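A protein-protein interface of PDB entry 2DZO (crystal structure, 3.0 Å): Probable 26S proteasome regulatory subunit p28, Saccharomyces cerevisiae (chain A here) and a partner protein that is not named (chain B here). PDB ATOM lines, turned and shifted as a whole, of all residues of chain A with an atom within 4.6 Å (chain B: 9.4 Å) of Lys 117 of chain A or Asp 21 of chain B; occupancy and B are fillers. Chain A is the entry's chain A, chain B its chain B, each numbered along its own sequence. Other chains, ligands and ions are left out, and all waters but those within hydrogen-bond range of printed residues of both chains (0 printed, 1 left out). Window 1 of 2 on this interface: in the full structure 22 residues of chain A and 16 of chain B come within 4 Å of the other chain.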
ATOM      1  N   TRP A  73     -10.687  -7.695  -3.926  1.00  0.00           N
ATOM      2  CA  TRP A  73      -9.920  -6.471  -4.088  1.00  0.00           C
ATOM      3  C   TRP A  73     -10.704  -5.341  -3.473  1.00  0.00           C
ATOM      4  O   TRP A  73     -11.880  -5.119  -3.778  1.00  0.00           O
ATOM      5  CB  TRP A  73      -9.643  -6.171  -5.559  1.00  0.00           C
ATOM      6  CG  TRP A  73      -8.590  -7.048  -6.164  1.00  0.00           C
ATOM      7  CD1 TRP A  73      -8.632  -8.403  -6.305  1.00  0.00           C
ATOM      8  CD2 TRP A  73      -7.353  -6.619  -6.745  1.00  0.00           C
ATOM      9  NE1 TRP A  73      -7.499  -8.849  -6.944  1.00  0.00           N
ATOM     10  CE2 TRP A  73      -6.697  -7.775  -7.227  1.00  0.00           C
ATOM     11  CE3 TRP A  73      -6.737  -5.371  -6.909  1.00  0.00           C
ATOM     12  CZ2 TRP A  73      -5.452  -7.719  -7.866  1.00  0.00           C
ATOM     13  CZ3 TRP A  73      -5.505  -5.318  -7.541  1.00  0.00           C
ATOM     14  CH2 TRP A  73      -4.873  -6.488  -8.014  1.00  0.00           C
ATOM     15  N   SER A  81      -2.085  -1.415  -6.005  1.00  0.00           N
ATOM     16  CA  SER A  81      -1.606  -2.020  -7.241  1.00  0.00           C
ATOM     17  C   SER A  81      -1.294  -0.946  -8.270  1.00  0.00           C
ATOM     18  O   SER A  81      -0.306  -1.055  -8.989  1.00  0.00           O
ATOM     19  CB  SER A  81      -2.648  -2.967  -7.827  1.00  0.00           C
ATOM     20  OG  SER A  81      -2.395  -3.166  -9.210  1.00  0.00           O
ATOM     21  N   LEU A 113       1.108  -6.839  -4.564  1.00  0.00           N
ATOM     22  CA  LEU A 113       0.659  -5.926  -5.614  1.00  0.00           C
ATOM     23  C   LEU A 113       1.627  -4.766  -5.780  1.00  0.00           C
ATOM     24  O   LEU A 113       2.081  -4.486  -6.885  1.00  0.00           O
ATOM     25  CB  LEU A 113      -0.731  -5.391  -5.288  1.00  0.00           C
ATOM     26  CG  LEU A 113      -1.839  -6.439  -5.309  1.00  0.00           C
ATOM     27  CD1 LEU A 113      -3.172  -5.780  -5.033  1.00  0.00           C
ATOM     28  CD2 LEU A 113      -1.864  -7.122  -6.660  1.00  0.00           C
ATOM     29  N   ALA A 114       1.960  -4.107  -4.676  1.00  0.00           N
ATOM     30  CA  ALA A 114       2.893  -2.986  -4.720  1.00  0.00           C
ATOM     31  C   ALA A 114       4.276  -3.433  -5.193  1.00  0.00           C
ATOM     32  O   ALA A 114       4.759  -2.969  -6.225  1.00  0.00           O
ATOM     33  CB  ALA A 114       2.997  -2.339  -3.350  1.00  0.00           C
ATOM     34  N   VAL A 115       4.904  -4.330  -4.434  1.00  0.00           N
ATOM     35  CA  VAL A 115       6.237  -4.842  -4.764  1.00  0.00           C
ATOM     36  C   VAL A 115       6.348  -5.340  -6.212  1.00  0.00           C
ATOM     37  O   VAL A 115       7.199  -4.874  -6.975  1.00  0.00           O
ATOM     38  CB  VAL A 115       6.634  -5.994  -3.812  1.00  0.00           C
ATOM     39  CG1 VAL A 115       7.997  -6.540  -4.183  1.00  0.00           C
ATOM     40  CG2 VAL A 115       6.648  -5.500  -2.396  1.00  0.00           C
ATOM     41  N   GLY A 116       5.488  -6.289  -6.575  1.00  0.00           N
ATOM     42  CA  GLY A 116       5.501  -6.839  -7.916  1.00  0.00           C
ATOM     43  C   GLY A 116       5.673  -5.795  -8.999  1.00  0.00           C
ATOM     44  O   GLY A 116       6.535  -5.942  -9.865  1.00  0.00           O
ATOM     45  N   LYS A 117       4.856  -4.742  -8.949  1.00  0.00           N
ATOM     46  CA  LYS A 117       4.908  -3.664  -9.933  1.00  0.00           C
ATOM     47  C   LYS A 117       6.072  -2.691  -9.736  1.00  0.00           C
ATOM     48  O   LYS A 117       6.355  -1.880 -10.617  1.00  0.00           O
ATOM     49  CB  LYS A 117       3.591  -2.899  -9.942  1.00  0.00           C
ATOM     50  CG  LYS A 117       2.398  -3.757 -10.318  1.00  0.00           C
ATOM     51  CD  LYS A 117       1.255  -2.905 -10.894  1.00  0.00           C
ATOM     52  CE  LYS A 117      -0.019  -3.726 -11.126  1.00  0.00           C
ATOM     53  NZ  LYS A 117       0.289  -5.066 -11.711  1.00  0.00           N
ATOM     54  N   LYS A 118       6.734  -2.773  -8.581  1.00  0.00           N
ATOM     55  CA  LYS A 118       7.899  -1.938  -8.251  1.00  0.00           C
ATOM     56  C   LYS A 118       7.608  -0.538  -7.705  1.00  0.00           C
ATOM     57  O   LYS A 118       8.374   0.392  -7.965  1.00  0.00           O
ATOM     58  CB  LYS A 118       8.814  -1.788  -9.474  1.00  0.00           C
ATOM     59  CG  LYS A 118       9.251  -3.089 -10.138  1.00  0.00           C
ATOM     60  CD  LYS A 118      10.023  -2.790 -11.420  1.00  0.00           C
ATOM     61  CE  LYS A 118      10.424  -4.042 -12.186  1.00  0.00           C
ATOM     62  NZ  LYS A 118      11.138  -3.696 -13.456  1.00  0.00           N
ATOM     63  N   TRP A 119       6.528  -0.377  -6.947  1.00  0.00           N
ATOM     64  CA  TRP A 119       6.195   0.939  -6.392  1.00  0.00           C
ATOM     65  C   TRP A 119       6.926   1.165  -5.080  1.00  0.00           C
ATOM     66  O   TRP A 119       6.341   1.019  -4.014  1.00  0.00           O
ATOM     67  CB  TRP A 119       4.687   1.060  -6.151  1.00  0.00           C
ATOM     68  CG  TRP A 119       3.821   0.828  -7.366  1.00  0.00           C
ATOM     69  CD1 TRP A 119       2.555   0.326  -7.371  1.00  0.00           C
ATOM     70  CD2 TRP A 119       4.150   1.097  -8.743  1.00  0.00           C
ATOM     71  NE1 TRP A 119       2.074   0.261  -8.655  1.00  0.00           N
ATOM     72  CE2 TRP A 119       3.030   0.727  -9.517  1.00  0.00           C
ATOM     73  CE3 TRP A 119       5.278   1.611  -9.394  1.00  0.00           C
ATOM     74  CZ2 TRP A 119       3.006   0.854 -10.911  1.00  0.00           C
ATOM     75  CZ3 TRP A 119       5.251   1.737 -10.780  1.00  0.00           C
ATOM     76  CH2 TRP A 119       4.122   1.359 -11.521  1.00  0.00           C
ATOM     77  N   ARG A 146       8.051 -11.930  -5.253  1.00  0.00           N
ATOM     78  CA  ARG A 146       7.716 -11.003  -6.316  1.00  0.00           C
ATOM     79  C   ARG A 146       8.946 -10.162  -6.642  1.00  0.00           C
ATOM     80  O   ARG A 146       9.433 -10.170  -7.776  1.00  0.00           O
ATOM     81  CB  ARG A 146       6.538 -10.115  -5.902  1.00  0.00           C
ATOM     82  CG  ARG A 146       5.174 -10.610  -6.395  1.00  0.00           C
ATOM     83  CD  ARG A 146       4.045  -9.775  -5.782  1.00  0.00           C
ATOM     84  NE  ARG A 146       2.868  -9.630  -6.645  1.00  0.00           N
ATOM     85  CZ  ARG A 146       2.028 -10.612  -6.956  1.00  0.00           C
ATOM     86  NH1 ARG A 146       2.217 -11.834  -6.478  1.00  0.00           N
ATOM     87  NH2 ARG A 146       0.999 -10.374  -7.749  1.00  0.00           N
ATOM     88  N   LEU B  16      -5.877  -4.020 -20.228  1.00  0.00           N
ATOM     89  CA  LEU B  16      -5.917  -4.437 -18.835  1.00  0.00           C
ATOM     90  C   LEU B  16      -6.179  -3.286 -17.874  1.00  0.00           C
ATOM     91  O   LEU B  16      -5.628  -2.198 -18.034  1.00  0.00           O
ATOM     92  CB  LEU B  16      -4.596  -5.114 -18.462  1.00  0.00           C
ATOM     93  CG  LEU B  16      -4.562  -6.633 -18.599  1.00  0.00           C
ATOM     94  CD1 LEU B  16      -5.092  -7.029 -19.953  1.00  0.00           C
ATOM     95  CD2 LEU B  16      -3.151  -7.136 -18.399  1.00  0.00           C
ATOM     96  N   ALA B  17      -7.022  -3.534 -16.876  1.00  0.00           N
ATOM     97  CA  ALA B  17      -7.325  -2.528 -15.875  1.00  0.00           C
ATOM     98  C   ALA B  17      -6.030  -2.058 -15.249  1.00  0.00           C
ATOM     99  O   ALA B  17      -5.135  -2.850 -14.950  1.00  0.00           O
ATOM    100  CB  ALA B  17      -8.220  -3.102 -14.808  1.00  0.00           C
ATOM    101  N   PRO B  18      -5.906  -0.752 -15.039  1.00  0.00           N
ATOM    102  CA  PRO B  18      -4.680  -0.222 -14.436  1.00  0.00           C
ATOM    103  C   PRO B  18      -4.181  -1.036 -13.237  1.00  0.00           C
ATOM    104  O   PRO B  18      -2.973  -1.215 -13.056  1.00  0.00           O
ATOM    105  CB  PRO B  18      -5.069   1.214 -14.067  1.00  0.00           C
ATOM    106  CG  PRO B  18      -6.593   1.168 -13.980  1.00  0.00           C
ATOM    107  CD  PRO B  18      -6.951   0.279 -15.132  1.00  0.00           C
ATOM    108  N   GLU B  19      -5.109  -1.544 -12.431  1.00  0.00           N
ATOM    109  CA  GLU B  19      -4.736  -2.327 -11.255  1.00  0.00           C
ATOM    110  C   GLU B  19      -4.574  -3.824 -11.518  1.00  0.00           C
ATOM    111  O   GLU B  19      -4.296  -4.587 -10.603  1.00  0.00           O
ATOM    112  CB  GLU B  19      -5.754  -2.122 -10.123  1.00  0.00           C
ATOM    113  CG  GLU B  19      -6.988  -3.006 -10.214  1.00  0.00           C
ATOM    114  CD  GLU B  19      -8.053  -2.436 -11.115  1.00  0.00           C
ATOM    115  OE1 GLU B  19      -9.001  -3.176 -11.473  1.00  0.00           O
ATOM    116  OE2 GLU B  19      -7.938  -1.239 -11.450  1.00  0.00           O
ATOM    117  N   ALA B  20      -4.755  -4.251 -12.758  1.00  0.00           N
ATOM    118  CA  ALA B  20      -4.605  -5.662 -13.060  1.00  0.00           C
ATOM    119  C   ALA B  20      -3.235  -6.069 -12.562  1.00  0.00           C
ATOM    120  O   ALA B  20      -2.363  -5.222 -12.363  1.00  0.00           O
ATOM    121  CB  ALA B  20      -4.726  -5.906 -14.547  1.00  0.00           C
ATOM    122  N   ASP B  21      -3.057  -7.367 -12.350  1.00  0.00           N
ATOM    123  CA  ASP B  21      -1.797  -7.902 -11.837  1.00  0.00           C
ATOM    124  C   ASP B  21      -1.426  -9.187 -12.570  1.00  0.00           C
ATOM    125  O   ASP B  21      -1.434 -10.276 -12.012  1.00  0.00           O
ATOM    126  CB  ASP B  21      -1.948  -8.146 -10.333  1.00  0.00           C
ATOM    127  CG  ASP B  21      -0.821  -8.957  -9.742  1.00  0.00           C
ATOM    128  OD1 ASP B  21       0.364  -8.666 -10.020  1.00  0.00           O
ATOM    129  OD2 ASP B  21      -1.139  -9.883  -8.967  1.00  0.00           O
ATOM    130  N   LEU B  22      -1.086  -9.025 -13.839  1.00  0.00           N
ATOM    131  CA  LEU B  22      -0.742 -10.140 -14.696  1.00  0.00           C
ATOM    132  C   LEU B  22       0.540 -10.826 -14.232  1.00  0.00           C
ATOM    133  O   LEU B  22       0.751 -12.014 -14.507  1.00  0.00           O
ATOM    134  CB  LEU B  22      -0.558  -9.651 -16.125  1.00  0.00           C
ATOM    135  CG  LEU B  22      -0.501 -10.706 -17.225  1.00  0.00           C
ATOM    136  CD1 LEU B  22      -1.775 -11.519 -17.190  1.00  0.00           C
ATOM    137  CD2 LEU B  22      -0.330 -10.040 -18.567  1.00  0.00           C
ATOM    138  N   ASP B  23       1.385 -10.098 -13.499  1.00  0.00           N
ATOM    139  CA  ASP B  23       2.669 -10.645 -13.028  1.00  0.00           C
ATOM    140  C   ASP B  23       2.458 -11.841 -12.137  1.00  0.00           C
ATOM    141  O   ASP B  23       3.153 -12.857 -12.192  1.00  0.00           O
ATOM    142  CB  ASP B  23       3.492  -9.576 -12.280  1.00  0.00           C
ATOM    143  CG  ASP B  23       2.733  -8.270 -12.063  1.00  0.00           C
ATOM    144  OD1 ASP B  23       1.966  -7.876 -12.951  1.00  0.00           O
ATOM    145  OD2 ASP B  23       2.946  -7.656 -11.004  1.00  0.00           O
ATOM    146  N   SER B  24       1.475 -11.687 -11.283  1.00  0.00           N
ATOM    147  CA  SER B  24       1.132 -12.741 -10.370  1.00  0.00           C
ATOM    148  C   SER B  24       0.915 -14.016 -11.192  1.00  0.00           C
ATOM    149  O   SER B  24       1.423 -15.099 -10.874  1.00  0.00           O
ATOM    150  CB  SER B  24      -0.155 -12.392  -9.646  1.00  0.00           C
ATOM    151  OG  SER B  24      -1.223 -12.428 -10.556  1.00  0.00           O
ATOM    152  N   LEU B  25       0.167 -13.866 -12.275  1.00  0.00           N
ATOM    153  CA  LEU B  25      -0.196 -14.975 -13.146  1.00  0.00           C
ATOM    154  C   LEU B  25       0.958 -15.705 -13.818  1.00  0.00           C
ATOM    155  O   LEU B  25       0.893 -16.916 -14.000  1.00  0.00           O
ATOM    156  CB  LEU B  25      -1.204 -14.474 -14.190  1.00  0.00           C
ATOM    157  CG  LEU B  25      -2.383 -15.420 -14.456  1.00  0.00           C
ATOM    158  CD1 LEU B  25      -3.444 -14.735 -15.272  1.00  0.00           C
ATOM    159  CD2 LEU B  25      -1.929 -16.674 -15.170  1.00  0.00           C
ATOM    160  N   ILE B  26       2.004 -14.971 -14.176  1.00  0.00           N
ATOM    161  CA  ILE B  26       3.167 -15.560 -14.825  1.00  0.00           C
ATOM    162  C   ILE B  26       4.114 -16.230 -13.810  1.00  0.00           C
ATOM    163  O   ILE B  26       4.631 -17.328 -14.027  1.00  0.00           O
ATOM    164  CB  ILE B  26       3.961 -14.478 -15.609  1.00  0.00           C
ATOM    165  CG1 ILE B  26       4.394 -13.375 -14.633  1.00  0.00           C
ATOM    166  CG2 ILE B  26       3.080 -13.819 -16.679  1.00  0.00           C
ATOM    167  CD1 ILE B  26       5.640 -12.551 -15.026  1.00  0.00           C
ATOM    168  N   ILE B  27       4.304 -15.551 -12.687  1.00  0.00           N
ATOM    169  CA  ILE B  27       5.200 -15.970 -11.622  1.00  0.00           C
ATOM    170  C   ILE B  27       4.847 -17.246 -10.865  1.00  0.00           C
ATOM    171  O   ILE B  27       5.658 -17.766 -10.099  1.00  0.00           O
ATOM    172  CB  ILE B  27       5.398 -14.788 -10.649  1.00  0.00           C
ATOM    173  CG1 ILE B  27       6.352 -13.786 -11.297  1.00  0.00           C
ATOM    174  CG2 ILE B  27       5.934 -15.253  -9.328  1.00  0.00           C
ATOM    175  CD1 ILE B  27       6.447 -12.444 -10.597  1.00  0.00           C
ATOM    176  N   ARG B  28       3.656 -17.779 -11.097  1.00  0.00           N
ATOM    177  CA  ARG B  28       3.251 -19.004 -10.413  1.00  0.00           C
ATOM    178  C   ARG B  28       4.155 -20.172 -10.754  1.00  0.00           C
ATOM    179  O   ARG B  28       4.943 -20.604  -9.913  1.00  0.00           O
ATOM    180  CB  ARG B  28       1.792 -19.307 -10.725  1.00  0.00           C
ATOM    181  CG  ARG B  28       0.937 -18.213 -10.150  1.00  0.00           C
ATOM    182  CD  ARG B  28      -0.409 -18.047 -10.794  1.00  0.00           C
ATOM    183  NE  ARG B  28      -0.970 -16.761 -10.388  1.00  0.00           N
ATOM    184  CZ  ARG B  28      -2.246 -16.422 -10.518  1.00  0.00           C
ATOM    185  NH1 ARG B  28      -3.111 -17.280 -11.045  1.00  0.00           N
ATOM    186  NH2 ARG B  28      -2.651 -15.223 -10.126  1.00  0.00           N
ATOM    187  N   MET B  41      -4.865 -15.313 -22.014  1.00  0.00           N
ATOM    188  CA  MET B  41      -5.185 -13.925 -22.311  1.00  0.00           C
ATOM    189  C   MET B  41      -6.464 -13.770 -23.048  1.00  0.00           C
ATOM    190  O   MET B  41      -7.224 -12.859 -22.773  1.00  0.00           O
ATOM    191  CB  MET B  41      -4.081 -13.248 -23.115  1.00  0.00           C
ATOM    192  CG  MET B  41      -2.927 -12.745 -22.275  1.00  0.00           C
ATOM    193  SD  MET B  41      -3.506 -11.954 -20.764  1.00  0.00           S
ATOM    194  CE  MET B  41      -4.663 -10.717 -21.452  1.00  0.00           C
ATOM    195  N   ILE B  56     -10.042  -5.271 -18.541  1.00  0.00           N
ATOM    196  CA  ILE B  56      -9.959  -6.581 -17.897  1.00  0.00           C
ATOM    197  C   ILE B  56      -9.581  -6.511 -16.419  1.00  0.00           C
ATOM    198  O   ILE B  56      -8.643  -5.810 -16.033  1.00  0.00           O
ATOM    199  CB  ILE B  56      -8.933  -7.487 -18.625  1.00  0.00           C
ATOM    200  CG1 ILE B  56      -9.449  -7.849 -20.023  1.00  0.00           C
ATOM    201  CG2 ILE B  56      -8.669  -8.733 -17.804  1.00  0.00           C
ATOM    202  CD1 ILE B  56      -8.533  -8.765 -20.818  1.00  0.00           C
ATOM    203  N   LEU B  57     -10.317  -7.256 -15.599  1.00  0.00           N
ATOM    204  CA  LEU B  57     -10.077  -7.291 -14.167  1.00  0.00           C
ATOM    205  C   LEU B  57      -9.344  -8.561 -13.810  1.00  0.00           C
ATOM    206  O   LEU B  57      -9.237  -9.473 -14.633  1.00  0.00           O
ATOM    207  CB  LEU B  57     -11.394  -7.221 -13.401  1.00  0.00           C
ATOM    208  CG  LEU B  57     -12.241  -5.986 -13.708  1.00  0.00           C
ATOM    209  CD1 LEU B  57     -13.389  -5.882 -12.712  1.00  0.00           C
ATOM    210  CD2 LEU B  57     -11.367  -4.747 -13.624  1.00  0.00           C
ATOM    211  N   GLN B  58      -8.832  -8.605 -12.582  1.00  0.00           N
ATOM    212  CA  GLN B  58      -8.091  -9.759 -12.098  1.00  0.00           C
ATOM    213  C   GLN B  58      -8.989 -10.952 -12.114  1.00  0.00           C
ATOM    214  O   GLN B  58      -8.548 -12.046 -12.405  1.00  0.00           O
ATOM    215  CB  GLN B  58      -7.577  -9.528 -10.678  1.00  0.00           C
ATOM    216  CG  GLN B  58      -6.110  -9.160 -10.602  1.00  0.00           C
ATOM    217  CD  GLN B  58      -5.219 -10.245 -11.170  1.00  0.00           C
ATOM    218  OE1 GLN B  58      -5.691 -11.336 -11.499  1.00  0.00           O
ATOM    219  NE2 GLN B  58      -3.923  -9.958 -11.283  1.00  0.00           N
ATOM    220  N   SER B  59     -10.258 -10.734 -11.805  1.00  0.00           N
ATOM    221  CA  SER B  59     -11.234 -11.824 -11.794  1.00  0.00           C
ATOM    222  C   SER B  59     -11.134 -12.662 -13.065  1.00  0.00           C
ATOM    223  O   SER B  59     -11.021 -13.887 -13.009  1.00  0.00           O
ATOM    224  CB  SER B  59     -12.661 -11.271 -11.668  1.00  0.00           C
ATOM    225  OG  SER B  59     -13.370 -11.372 -12.891  1.00  0.00           O
ATOM    226  N   LEU B  61      -8.705 -12.866 -15.352  1.00  0.00           N
ATOM    227  CA  LEU B  61      -7.421 -13.527 -15.532  1.00  0.00           C
ATOM    228  C   LEU B  61      -7.225 -14.826 -14.770  1.00  0.00           C
ATOM    229  O   LEU B  61      -6.746 -15.808 -15.330  1.00  0.00           O
ATOM    230  CB  LEU B  61      -6.314 -12.545 -15.182  1.00  0.00           C
ATOM    231  CG  LEU B  61      -6.419 -11.247 -15.990  1.00  0.00           C
ATOM    232  CD1 LEU B  61      -6.357 -10.102 -15.029  1.00  0.00           C
ATOM    233  CD2 LEU B  61      -5.315 -11.129 -17.040  1.00  0.00           C
ATOM    234  N   GLU B  62      -7.587 -14.817 -13.491  1.00  0.00           N
ATOM    235  CA  GLU B  62      -7.470 -15.976 -12.615  1.00  0.00           C
ATOM    236  C   GLU B  62      -8.390 -17.037 -13.128  1.00  0.00           C
ATOM    237  O   GLU B  62      -8.055 -18.212 -13.134  1.00  0.00           O
ATOM    238  CB  GLU B  62      -7.902 -15.609 -11.213  1.00  0.00           C
ATOM    239  CG  GLU B  62      -7.110 -14.477 -10.603  1.00  0.00           C
ATOM    240  CD  GLU B  62      -5.633 -14.782 -10.543  1.00  0.00           C
ATOM    241  OE1 GLU B  62      -5.288 -15.981 -10.453  1.00  0.00           O
ATOM    242  OE2 GLU B  62      -4.824 -13.828 -10.577  1.00  0.00           O
ATOM    243  N   TYR B  65      -6.687 -18.317 -16.257  1.00  0.00           N
ATOM    244  CA  TYR B  65      -5.559 -19.166 -15.900  1.00  0.00           C
ATOM    245  C   TYR B  65      -6.070 -20.570 -15.600  1.00  0.00           C
ATOM    246  O   TYR B  65      -5.539 -21.554 -16.101  1.00  0.00           O
ATOM    247  CB  TYR B  65      -4.858 -18.582 -14.672  1.00  0.00           C
ATOM    248  CG  TYR B  65      -3.557 -19.249 -14.285  1.00  0.00           C
ATOM    249  CD1 TYR B  65      -2.570 -19.499 -15.236  1.00  0.00           C
ATOM    250  CD2 TYR B  65      -3.285 -19.564 -12.953  1.00  0.00           C
ATOM    251  CE1 TYR B  65      -1.341 -20.036 -14.877  1.00  0.00           C
ATOM    252  CE2 TYR B  65      -2.058 -20.105 -12.579  1.00  0.00           C
ATOM    253  CZ  TYR B  65      -1.089 -20.339 -13.550  1.00  0.00           C
ATOM    254  OH  TYR B  65       0.132 -20.878 -13.203  1.00  0.00           O
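The side-chain hydroxyl of Ser 81 of chain A lies within hydrogen-bond range of the backbone carbonyl oxygen of Glu 19 of chain B, at 2.8 Å.
NZ of Lys 117 of chain A sits at hydrogen-bond distance from O of Ala 20 of chain B, 2.7 Å away.
NZ of Lys 117 of chain A is in salt-bridge range of OD1 of Asp 21 of chain B (3.98 Å).
NZ of Lys 117 of chain A is in salt-bridge range of OD1 of Asp 23 of chain B (3.5 Å).
NH2 of Arg 146 of chain A is in salt-bridge range of OD2 of Asp 21 of chain B, at 2.5 Å.
O of Ser 81 of chain A is in hydrogen-bond range of NE1 of Trp 119 of chain A (2.7 Å).
The side-chain hydroxyl of Ser 24 of chain B sits at hydrogen-bond distance from the backbone carbonyl oxygen of Asp 21 of chain B (2.6 Å).
NE2 of Gln 58 of chain B sits at hydrogen-bond distance from O of Asp 21 of chain B.
The backbone carbonyl oxygen (O) of Ser 24 of chain B lies within hydrogen-bond range of the guanidinium group (NE) of Arg 28 of chain B (3.0 Å).
OE2 of Glu 62 of chain B lies close to OE1 of Gln 58 of chain B (2.8 Å).
Among the printed residues, merely in contact across the chains: Arg 146 of chain A with Ser 24 of chain B, Trp 73 of chain A with Gln 58 of chain B, Trp 73 of chain A with Glu 19 of chain B, Leu 113 of chain A with Asp 21 of chain B, Ser 81 of chain A with Ala 20 of chain B and Gly 116 of chain A with Asp 23 of chain B.
Printed residues of chain B within 4 Å of Gly 116 of chain A: Asp 23.
Of chain B, only Ala 20, Asp 21 and Asp 23 come within 4 Å of Lys 117 of chain A.
Of the printed residues of chain A, Glu 19 of chain B touches Trp 73 and Ser 81.
Of the printed residues of chain A, Ala 20 of chain B touches Ser 81 (3.8 Å) and Lys 117 (2.7 Å).
Of chain A, only Leu 113 (3.7 Å), Lys 117 (3.5 Å) and Arg 146 (2.5 Å) come within 4 Å of Asp 21 of chain B.
The nearest residue of chain B that does not touch Lys 117 of chain A is Pro 18 of chain B (4.3 Å).
The nearest residue of chain A that does not touch Asp 21 of chain B is Trp 73 of chain A (4.1 Å).
The nearest printed residue of chain A that does not touch Glu 19 of chain B is Lys 117 of chain A (4.4 Å).
Of the 21 printed residues of chain B, 6 touch a printed residue of chain A.
Of the 10 printed residues of chain A, 6 touch a printed residue of chain B.
Along chain A the printed residues that touch a printed residue of chain B span positions 73 to 146.
Among the printed residues, 11 pairs touch across the chains.
Among the printed residues, Asp or Glu carboxylates within 4 Å of a Lys or Arg side-chain nitrogen of the other chain: Lys 117 of chain A with Asp 21 of chain B (3.98 Å), Lys 117 of chain A with Asp 23 of chain B (3.5 Å) and Arg 146 of chain A with Asp 21 of chain B (2.5 Å).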
